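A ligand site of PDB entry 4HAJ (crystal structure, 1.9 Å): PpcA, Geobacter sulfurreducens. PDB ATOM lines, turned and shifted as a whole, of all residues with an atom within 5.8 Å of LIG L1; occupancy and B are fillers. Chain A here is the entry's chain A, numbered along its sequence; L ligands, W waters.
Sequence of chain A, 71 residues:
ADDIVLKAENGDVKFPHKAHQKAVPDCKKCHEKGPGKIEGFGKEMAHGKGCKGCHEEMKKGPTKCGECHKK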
ATOM      1  N   ALA A   1     -16.672  10.597 -12.464  1.00  0.00           N
ATOM      2  CA  ALA A   1     -15.438  10.955 -13.208  1.00  0.00           C
ATOM      3  C   ALA A   1     -14.285  11.212 -12.242  1.00  0.00           C
ATOM      4  O   ALA A   1     -14.495  11.372 -11.042  1.00  0.00           O
ATOM      5  CB  ALA A   1     -15.688  12.183 -14.083  1.00  0.00           C
ATOM      6  N   ASP A   2     -13.078  11.293 -12.775  1.00  0.00           N
ATOM      7  CA  ASP A   2     -11.882  11.431 -11.963  1.00  0.00           C
ATOM      8  C   ASP A   2     -11.445  12.866 -11.768  1.00  0.00           C
ATOM      9  O   ASP A   2     -11.724  13.721 -12.594  1.00  0.00           O
ATOM     10  CB  ASP A   2     -10.736  10.694 -12.635  1.00  0.00           C
ATOM     11  CG  ASP A   2     -10.999   9.238 -12.743  1.00  0.00           C
ATOM     12  OD1 ASP A   2     -11.268   8.607 -11.670  1.00  0.00           O
ATOM     13  OD2 ASP A   2     -10.951   8.645 -13.842  1.00  0.00           O
ATOM     14  N   ASP A   3     -10.700  13.085 -10.688  1.00  0.00           N
ATOM     15  CA  ASP A   3     -10.044  14.376 -10.462  1.00  0.00           C
ATOM     16  C   ASP A   3      -9.000  14.573 -11.505  1.00  0.00           C
ATOM     17  O   ASP A   3      -8.581  13.621 -12.171  1.00  0.00           O
ATOM     18  CB  ASP A   3      -9.402  14.444  -9.071  1.00  0.00           C
ATOM     19  CG  ASP A   3     -10.437  14.579  -7.980  1.00  0.00           C
ATOM     20  OD1 ASP A   3     -11.575  14.999  -8.265  1.00  0.00           O
ATOM     21  OD2 ASP A   3     -10.181  14.290  -6.804  1.00  0.00           O
ATOM     22  N   ILE A   4      -8.595  15.811 -11.697  1.00  0.00           N
ATOM     23  CA  ILE A   4      -7.538  16.058 -12.645  1.00  0.00           C
ATOM     24  C   ILE A   4      -6.353  16.711 -11.976  1.00  0.00           C
ATOM     25  O   ILE A   4      -6.482  17.263 -10.904  1.00  0.00           O
ATOM     26  CB  ILE A   4      -8.065  16.847 -13.840  1.00  0.00           C
ATOM     27  CG1 ILE A   4      -8.474  18.240 -13.460  1.00  0.00           C
ATOM     28  CG2 ILE A   4      -9.228  16.088 -14.455  1.00  0.00           C
ATOM     29  CD1 ILE A   4      -9.121  18.943 -14.646  1.00  0.00           C
ATOM     30  N   PHE A  15      -6.522  18.835  -8.315  1.00  0.00           N
ATOM     31  CA  PHE A  15      -7.805  19.521  -8.174  1.00  0.00           C
ATOM     32  C   PHE A  15      -8.822  18.511  -7.677  1.00  0.00           C
ATOM     33  O   PHE A  15      -9.323  17.721  -8.468  1.00  0.00           O
ATOM     34  CB  PHE A  15      -8.295  20.131  -9.483  1.00  0.00           C
ATOM     35  CG  PHE A  15      -9.648  20.761  -9.352  1.00  0.00           C
ATOM     36  CD1 PHE A  15      -9.800  21.971  -8.663  1.00  0.00           C
ATOM     37  CD2 PHE A  15     -10.770  20.097  -9.792  1.00  0.00           C
ATOM     38  CE1 PHE A  15     -11.045  22.543  -8.494  1.00  0.00           C
ATOM     39  CE2 PHE A  15     -12.034  20.650  -9.611  1.00  0.00           C
ATOM     40  CZ  PHE A  15     -12.172  21.870  -8.955  1.00  0.00           C
ATOM     41  N   PRO A  16      -9.101  18.505  -6.381  1.00  0.00           N
ATOM     42  CA  PRO A  16     -10.034  17.529  -5.819  1.00  0.00           C
ATOM     43  C   PRO A  16     -11.483  18.021  -5.905  1.00  0.00           C
ATOM     44  O   PRO A  16     -11.852  18.979  -5.239  1.00  0.00           O
ATOM     45  CB  PRO A  16      -9.558  17.392  -4.377  1.00  0.00           C
ATOM     46  CG  PRO A  16      -8.920  18.714  -4.035  1.00  0.00           C
ATOM     47  CD  PRO A  16      -8.517  19.368  -5.343  1.00  0.00           C
ATOM     48  N   HIS A  17     -12.304  17.369  -6.741  1.00  0.00           N
ATOM     49  CA  HIS A  17     -13.632  17.923  -6.981  1.00  0.00           C
ATOM     50  C   HIS A  17     -14.529  17.805  -5.753  1.00  0.00           C
ATOM     51  O   HIS A  17     -15.289  18.735  -5.453  1.00  0.00           O
ATOM     52  CB  HIS A  17     -14.327  17.308  -8.181  1.00  0.00           C
ATOM     53  CG  HIS A  17     -15.620  17.989  -8.522  1.00  0.00           C
ATOM     54  ND1 HIS A  17     -16.851  17.514  -8.108  1.00  0.00           N
ATOM     55  CD2 HIS A  17     -15.872  19.134  -9.193  1.00  0.00           C
ATOM     56  CE1 HIS A  17     -17.796  18.319  -8.544  1.00  0.00           C
ATOM     57  NE2 HIS A  17     -17.231  19.308  -9.207  1.00  0.00           N
ATOM     58  N   HIS A  20     -14.592  20.635  -3.421  1.00  0.00           N
ATOM     59  CA  HIS A  20     -15.119  21.848  -4.024  1.00  0.00           C
ATOM     60  C   HIS A  20     -16.636  21.844  -4.115  1.00  0.00           C
ATOM     61  O   HIS A  20     -17.266  22.863  -3.823  1.00  0.00           O
ATOM     62  CB  HIS A  20     -14.471  22.100  -5.387  1.00  0.00           C
ATOM     63  CG  HIS A  20     -13.059  22.587  -5.244  1.00  0.00           C
ATOM     64  ND1 HIS A  20     -11.988  21.733  -5.140  1.00  0.00           N
ATOM     65  CD2 HIS A  20     -12.568  23.840  -5.091  1.00  0.00           C
ATOM     66  CE1 HIS A  20     -10.881  22.453  -4.996  1.00  0.00           C
ATOM     67  NE2 HIS A  20     -11.205  23.729  -4.945  1.00  0.00           N
ATOM     68  N   GLN A  21     -17.208  20.705  -4.505  1.00  0.00           N
ATOM     69  CA  GLN A  21     -18.668  20.575  -4.546  1.00  0.00           C
ATOM     70  C   GLN A  21     -19.300  20.868  -3.177  1.00  0.00           C
ATOM     71  O   GLN A  21     -20.363  21.531  -3.080  1.00  0.00           O
ATOM     72  CB  GLN A  21     -19.037  19.155  -5.002  1.00  0.00           C
ATOM     73  CG  GLN A  21     -20.506  18.995  -5.341  1.00  0.00           C
ATOM     74  CD  GLN A  21     -20.829  17.680  -6.040  1.00  0.00           C
ATOM     75  OE1 GLN A  21     -21.985  17.281  -6.092  1.00  0.00           O
ATOM     76  NE2 GLN A  21     -19.817  17.007  -6.563  1.00  0.00           N
ATOM     77  N   LYS A  22     -18.638  20.374  -2.127  1.00  0.00           N
ATOM     78  CA  LYS A  22     -19.092  20.549  -0.755  1.00  0.00           C
ATOM     79  C   LYS A  22     -18.925  21.989  -0.240  1.00  0.00           C
ATOM     80  O   LYS A  22     -19.833  22.549   0.404  1.00  0.00           O
ATOM     81  CB  LYS A  22     -18.353  19.582   0.166  1.00  0.00           C
ATOM     82  CG  LYS A  22     -18.668  19.801   1.634  1.00  0.00           C
ATOM     83  N   VAL A  24     -18.228  24.858  -2.052  1.00  0.00           N
ATOM     84  CA  VAL A  24     -18.645  25.920  -2.967  1.00  0.00           C
ATOM     85  C   VAL A  24     -20.031  25.524  -3.551  1.00  0.00           C
ATOM     86  O   VAL A  24     -20.161  25.180  -4.731  1.00  0.00           O
ATOM     87  CB  VAL A  24     -17.589  26.147  -4.105  1.00  0.00           C
ATOM     88  CG1 VAL A  24     -17.942  27.366  -4.970  1.00  0.00           C
ATOM     89  CG2 VAL A  24     -16.179  26.304  -3.506  1.00  0.00           C
ATOM     90  N   PRO A  25     -21.058  25.596  -2.709  1.00  0.00           N
ATOM     91  CA  PRO A  25     -22.442  25.311  -3.146  1.00  0.00           C
ATOM     92  C   PRO A  25     -22.963  26.175  -4.290  1.00  0.00           C
ATOM     93  O   PRO A  25     -23.903  25.788  -4.990  1.00  0.00           O
ATOM     94  CB  PRO A  25     -23.267  25.557  -1.864  1.00  0.00           C
ATOM     95  CG  PRO A  25     -22.406  26.313  -0.967  1.00  0.00           C
ATOM     96  CD  PRO A  25     -20.992  25.913  -1.273  1.00  0.00           C
ATOM     97  N   ASP A  26     -22.370  27.351  -4.477  1.00  0.00           N
ATOM     98  CA  ASP A  26     -22.627  28.163  -5.643  1.00  0.00           C
ATOM     99  C   ASP A  26     -21.851  27.570  -6.857  1.00  0.00           C
ATOM    100  O   ASP A  26     -20.780  28.046  -7.248  1.00  0.00           O
ATOM    101  CB  ASP A  26     -22.250  29.620  -5.374  1.00  0.00           C
ATOM    102  CG  ASP A  26     -22.560  30.544  -6.539  1.00  0.00           C
ATOM    103  OD1 ASP A  26     -23.309  30.145  -7.469  1.00  0.00           O
ATOM    104  OD2 ASP A  26     -22.047  31.678  -6.644  1.00  0.00           O
ATOM    105  N   CYS A  27     -22.449  26.554  -7.451  1.00  0.00           N
ATOM    106  CA  CYS A  27     -21.841  25.795  -8.541  1.00  0.00           C
ATOM    107  C   CYS A  27     -21.511  26.687  -9.712  1.00  0.00           C
ATOM    108  O   CYS A  27     -20.563  26.432 -10.444  1.00  0.00           O
ATOM    109  CB  CYS A  27     -22.766  24.679  -9.009  1.00  0.00           C
ATOM    110  SG  CYS A  27     -23.381  23.616  -7.688  1.00  0.00           S
ATOM    111  N   LYS A  29     -20.068  29.315  -9.821  1.00  0.00           N
ATOM    112  CA  LYS A  29     -18.732  29.884  -9.749  1.00  0.00           C
ATOM    113  C   LYS A  29     -17.825  29.284 -10.773  1.00  0.00           C
ATOM    114  O   LYS A  29     -16.948  29.952 -11.273  1.00  0.00           O
ATOM    115  CB  LYS A  29     -18.138  29.721  -8.354  1.00  0.00           C
ATOM    116  CG  LYS A  29     -18.709  30.688  -7.350  1.00  0.00           C
ATOM    117  CD  LYS A  29     -18.419  32.096  -7.765  1.00  0.00           C
ATOM    118  CE  LYS A  29     -18.286  33.035  -6.610  1.00  0.00           C
ATOM    119  NZ  LYS A  29     -17.557  34.262  -7.074  1.00  0.00           N
ATOM    120  N   CYS A  30     -18.060  28.020 -11.118  1.00  0.00           N
ATOM    121  CA  CYS A  30     -17.244  27.324 -12.110  1.00  0.00           C
ATOM    122  C   CYS A  30     -18.017  26.763 -13.283  1.00  0.00           C
ATOM    123  O   CYS A  30     -17.457  26.614 -14.373  1.00  0.00           O
ATOM    124  CB  CYS A  30     -16.561  26.177 -11.413  1.00  0.00           C
ATOM    125  SG  CYS A  30     -15.394  26.734 -10.178  1.00  0.00           S
ATOM    126  N   HIS A  31     -19.289  26.415 -13.056  1.00  0.00           N
ATOM    127  CA  HIS A  31     -20.087  25.711 -14.064  1.00  0.00           C
ATOM    128  C   HIS A  31     -21.061  26.643 -14.805  1.00  0.00           C
ATOM    129  O   HIS A  31     -21.407  27.709 -14.314  1.00  0.00           O
ATOM    130  CB  HIS A  31     -20.803  24.518 -13.434  1.00  0.00           C
ATOM    131  CG  HIS A  31     -19.870  23.417 -13.005  1.00  0.00           C
ATOM    132  ND1 HIS A  31     -18.990  22.798 -13.876  1.00  0.00           N
ATOM    133  CD2 HIS A  31     -19.666  22.839 -11.805  1.00  0.00           C
ATOM    134  CE1 HIS A  31     -18.294  21.886 -13.216  1.00  0.00           C
ATOM    135  NE2 HIS A  31     -18.699  21.871 -11.960  1.00  0.00           N
ATOM    136  N   GLY A  50      -9.210  32.011 -10.685  1.00  0.00           N
ATOM    137  CA  GLY A  50      -9.318  30.602 -11.054  1.00  0.00           C
ATOM    138  C   GLY A  50      -9.031  29.597  -9.953  1.00  0.00           C
ATOM    139  O   GLY A  50      -9.608  28.507  -9.935  1.00  0.00           O
HETATM  140 FE1  LIG L   1     -18.005  20.618 -10.566  1.00  0.00          FE
HETATM  141  C1  LIG L   1     -16.902  18.092 -12.526  1.00  0.00           C
HETATM  142  C2  LIG L   1     -21.170  19.297 -10.610  1.00  0.00           C
HETATM  143  C3  LIG L   1     -18.921  22.688  -8.034  1.00  0.00           C
HETATM  144  C4  LIG L   1     -15.266  22.446 -11.198  1.00  0.00           C
HETATM  145  N1  LIG L   1     -18.865  19.073 -11.467  1.00  0.00           N
HETATM  146  C5  LIG L   1     -18.200  18.062 -12.113  1.00  0.00           C
HETATM  147  C6  LIG L   1     -19.086  16.952 -12.300  1.00  0.00           C
HETATM  148  C7  LIG L   1     -20.264  17.268 -11.782  1.00  0.00           C
HETATM  149  C8  LIG L   1     -20.164  18.610 -11.249  1.00  0.00           C
HETATM  150  C9  LIG L   1     -21.545  16.367 -11.753  1.00  0.00           C
HETATM  151  C10 LIG L   1     -18.668  15.596 -12.921  1.00  0.00           C
HETATM  152  C11 LIG L   1     -18.229  14.814 -11.653  1.00  0.00           C
HETATM  153  C12 LIG L   1     -18.109  13.307 -11.762  1.00  0.00           C
HETATM  154  O1  LIG L   1     -18.783  12.690 -12.638  1.00  0.00           O
HETATM  155  O2  LIG L   1     -17.331  12.716 -10.943  1.00  0.00           O
HETATM  156  N2  LIG L   1     -19.735  20.907  -9.472  1.00  0.00           N
HETATM  157  C13 LIG L   1     -20.951  20.280  -9.678  1.00  0.00           C
HETATM  158  C14 LIG L   1     -21.908  20.859  -8.747  1.00  0.00           C
HETATM  159  C15 LIG L   1     -21.266  21.790  -8.024  1.00  0.00           C
HETATM  160  C16 LIG L   1     -19.892  21.836  -8.477  1.00  0.00           C
HETATM  161  C17 LIG L   1     -23.396  20.407  -8.637  1.00  0.00           C
HETATM  162  C18 LIG L   1     -21.769  22.701  -6.884  1.00  0.00           C
HETATM  163  C19 LIG L   1     -22.283  22.134  -5.789  1.00  0.00           C
HETATM  164  N3  LIG L   1     -17.248  22.270  -9.775  1.00  0.00           N
HETATM  165  C20 LIG L   1     -17.752  22.999  -8.713  1.00  0.00           C
HETATM  166  C21 LIG L   1     -16.858  24.114  -8.459  1.00  0.00           C
HETATM  167  C22 LIG L   1     -15.864  24.034  -9.340  1.00  0.00           C
HETATM  168  C23 LIG L   1     -16.077  22.874 -10.174  1.00  0.00           C
HETATM  169  C24 LIG L   1     -17.029  25.223  -7.412  1.00  0.00           C
HETATM  170  C25 LIG L   1     -14.669  25.000  -9.479  1.00  0.00           C
HETATM  171  C26 LIG L   1     -13.950  25.331  -8.380  1.00  0.00           C
HETATM  172  N4  LIG L   1     -16.377  20.326 -11.719  1.00  0.00           N
HETATM  173  C27 LIG L   1     -15.324  21.215 -11.792  1.00  0.00           C
HETATM  174  C28 LIG L   1     -14.281  20.621 -12.564  1.00  0.00           C
HETATM  175  C29 LIG L   1     -14.781  19.253 -12.984  1.00  0.00           C
HETATM  176  C30 LIG L   1     -16.100  19.181 -12.419  1.00  0.00           C
HETATM  177  C31 LIG L   1     -12.934  21.210 -12.945  1.00  0.00           C
HETATM  178  C32 LIG L   1     -14.037  18.203 -13.836  1.00  0.00           C
HETATM  179  C33 LIG L   1     -12.765  17.692 -13.134  1.00  0.00           C
HETATM  180  C34 LIG L   1     -13.083  16.883 -11.891  1.00  0.00           C
HETATM  181  O3  LIG L   1     -14.151  16.230 -11.873  1.00  0.00           O
HETATM  182  O4  LIG L   1     -12.230  16.914 -10.967  1.00  0.00           O
HETATM  183 FE1  LG2 L   2     -10.014  25.200  -4.282  1.00  0.00          FE
HETATM  184  C1  LG2 L   2      -9.985  23.708  -1.238  1.00  0.00           C
HETATM  185  C2  LG2 L   2      -7.185  23.473  -5.143  1.00  0.00           C
HETATM  186  C3  LG2 L   2     -10.190  26.498  -7.393  1.00  0.00           C
HETATM  187  C4  LG2 L   2     -12.666  27.171  -3.351  1.00  0.00           C
HETATM  188  N1  LG2 L   2      -8.791  23.844  -3.379  1.00  0.00           N
HETATM  189  C5  LG2 L   2      -8.993  23.325  -2.121  1.00  0.00           C
HETATM  190  C6  LG2 L   2      -8.009  22.292  -1.866  1.00  0.00           C
HETATM  191  C7  LG2 L   2      -7.227  22.225  -2.949  1.00  0.00           C
HETATM  192  C8  LG2 L   2      -7.710  23.196  -3.914  1.00  0.00           C
HETATM  193  C9  LG2 L   2      -6.027  21.279  -3.150  1.00  0.00           C
HETATM  194  C10 LG2 L   2      -7.873  21.478  -0.556  1.00  0.00           C
HETATM  195  C11 LG2 L   2      -9.008  20.459  -0.459  1.00  0.00           C
HETATM  196  C12 LG2 L   2      -8.938  19.714   0.853  1.00  0.00           C
HETATM  197  O1  LG2 L   2      -8.372  20.252   1.838  1.00  0.00           O
HETATM  198  O2  LG2 L   2      -9.453  18.569   0.874  1.00  0.00           O
HETATM  199  N2  LG2 L   2      -8.916  25.028  -5.933  1.00  0.00           N
HETATM  200  C13 LG2 L   2      -7.783  24.275  -6.089  1.00  0.00           C
HETATM  201  C14 LG2 L   2      -7.293  24.463  -7.427  1.00  0.00           C
HETATM  202  C15 LG2 L   2      -8.137  25.267  -8.066  1.00  0.00           C
HETATM  203  C16 LG2 L   2      -9.145  25.664  -7.116  1.00  0.00           C
HETATM  204  C17 LG2 L   2      -6.018  23.783  -7.966  1.00  0.00           C
HETATM  205  C18 LG2 L   2      -8.059  25.768  -9.526  1.00  0.00           C
HETATM  206  C19 LG2 L   2      -7.836  24.831 -10.479  1.00  0.00           C
HETATM  207  N3  LG2 L   2     -11.196  26.568  -5.200  1.00  0.00           N
HETATM  208  C20 LG2 L   2     -11.102  26.954  -6.515  1.00  0.00           C
HETATM  209  C21 LG2 L   2     -12.153  27.889  -6.807  1.00  0.00           C
HETATM  210  C22 LG2 L   2     -12.843  28.080  -5.679  1.00  0.00           C
HETATM  211  C23 LG2 L   2     -12.248  27.267  -4.653  1.00  0.00           C
HETATM  212  C24 LG2 L   2     -12.375  28.555  -8.164  1.00  0.00           C
HETATM  213  C25 LG2 L   2     -14.078  28.991  -5.475  1.00  0.00           C
HETATM  214  C26 LG2 L   2     -14.792  29.434  -6.531  1.00  0.00           C
HETATM  215  N4  LG2 L   2     -11.168  25.403  -2.590  1.00  0.00           N
HETATM  216  C27 LG2 L   2     -12.176  26.327  -2.397  1.00  0.00           C
HETATM  217  C28 LG2 L   2     -12.656  26.262  -1.023  1.00  0.00           C
HETATM  218  C29 LG2 L   2     -11.813  25.170  -0.402  1.00  0.00           C
HETATM  219  C30 LG2 L   2     -10.920  24.696  -1.431  1.00  0.00           C
HETATM  220  C31 LG2 L   2     -13.760  27.078  -0.325  1.00  0.00           C
HETATM  221  C32 LG2 L   2     -11.887  24.662   1.039  1.00  0.00           C
HETATM  222  C33 LG2 L   2     -12.394  23.231   0.989  1.00  0.00           C
HETATM  223  C34 LG2 L   2     -12.254  22.572   2.332  1.00  0.00           C
HETATM  224  O3  LG2 L   2     -11.259  22.821   3.051  1.00  0.00           O
HETATM  225  O4  LG2 L   2     -13.147  21.782   2.663  1.00  0.00           O
HETATM  226  C1  LG3 L   3      -7.590  23.501 -18.153  1.00  0.00           C
HETATM  227  C2  LG3 L   3      -7.697  23.482 -16.610  1.00  0.00           C
HETATM  228  C3  LG3 L   3      -8.915  22.629 -16.200  1.00  0.00           C
HETATM  229  C4  LG3 L   3     -10.259  23.178 -16.781  1.00  0.00           C
HETATM  230  C5  LG3 L   3     -10.104  23.313 -18.319  1.00  0.00           C
HETATM  231  C6  LG3 L   3      -8.869  24.142 -18.684  1.00  0.00           C
HETATM  232  C7  LG3 L   3      -8.951  22.505 -14.645  1.00  0.00           C
HETATM  233  C8  LG3 L   3      -9.363  23.845 -13.984  1.00  0.00           C
HETATM  234  C9  LG3 L   3     -10.686  24.410 -14.587  1.00  0.00           C
HETATM  235  C10 LG3 L   3     -10.617  24.512 -16.126  1.00  0.00           C
HETATM  236  C11 LG3 L   3     -10.985  25.832 -14.057  1.00  0.00           C
HETATM  237  C12 LG3 L   3     -12.353  26.359 -14.495  1.00  0.00           C
HETATM  238  C13 LG3 L   3     -12.303  26.502 -16.031  1.00  0.00           C
HETATM  239  C14 LG3 L   3     -11.940  25.147 -16.689  1.00  0.00           C
HETATM  240  C15 LG3 L   3     -11.029  25.964 -12.508  1.00  0.00           C
HETATM  241  C16 LG3 L   3     -11.994  27.149 -12.265  1.00  0.00           C
HETATM  242  C17 LG3 L   3     -12.395  27.667 -13.670  1.00  0.00           C
HETATM  243  C18 LG3 L   3     -11.367  22.158 -16.501  1.00  0.00           C
HETATM  244  C19 LG3 L   3     -13.752  28.395 -13.564  1.00  0.00           C
HETATM  245  O1  LG3 L   3     -11.311  27.439 -16.432  1.00  0.00           O
HETATM  246  O2  LG3 L   3      -6.472  24.317 -18.489  1.00  0.00           O
HETATM  247  C20 LG3 L   3     -13.492  25.426 -14.090  1.00  0.00           C
HETATM  248  C21 LG3 L   3     -13.723  29.548 -12.524  1.00  0.00           C
HETATM  249  C22 LG3 L   3     -12.686  30.622 -12.864  1.00  0.00           C
HETATM  250  C23 LG3 L   3     -13.272  31.749 -13.725  1.00  0.00           C
HETATM  251  O3  LG3 L   3     -14.204  32.429 -13.294  1.00  0.00           O
HETATM  252  O4  LG3 L   3     -12.784  31.985 -14.829  1.00  0.00           O
HETATM  253  C24 LG3 L   3     -14.267  28.886 -14.946  1.00  0.00           C
HETATM  254  O   HOH W   1     -19.935  10.409 -11.811  1.00  0.00           O
HETATM  255  O   HOH W   2     -14.061  14.260 -10.109  1.00  0.00           O
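An oxygen (O2) of LIG L1 sits at hydrogen-bond distance from the backbone NH (N) of Ala 1 (2.7 Å). C25 of LIG L1 is covalently linked to SG of Cys 30 (2.0 Å). NE2 of His 20 is bound to FE1 of LG2 L2, 2.0 Å away. C18 of LIG L1 is covalently linked to SG of Cys 27 (2.0 Å). FE1 of LIG L1 is bound by NE2 of His 17 (2.0 Å). An iron atom (FE1) of LIG L1 is bound by a ring nitrogen (NE2) of His 31.
The side-chain carboxylate (OD1) of Asp 3 is in hydrogen-bond range of the backbone NH (N) of His 17, 2.9 Å away. ND1 of His 17 lies close to NE2 of Gln 21, at 3.4 Å. N of Phe 15 is in hydrogen-bond range of O of Ile 4, 3.0 Å away. ND1 of His 20 lies within hydrogen-bond range of O of Pro 16 (2.8 Å).
OD1 of Asp 3 lies close to O4 of LIG L1, at 3.4 Å. Residues that only touch LIG L1: Asp 2, Ile 4, Phe 15, His 20, Gln 21 and Val 24. Hydrophobic or aromatic side chains that line LIG L1: Ala 1, Phe 15, His 17, His 20, Val 24 and His 31. 12 residues have an atom within 4 Å of LIG L1: Ala 1, Asp 2, Asp 3, Ile 4, Phe 15, His 17, His 20, Gln 21, Val 24, Cys 27, Cys 30 and His 31.
Water W1 bridges an oxygen (O1) of LIG L1 (2.7 Å) and the backbone NH of Ala 1 (3.3 Å).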
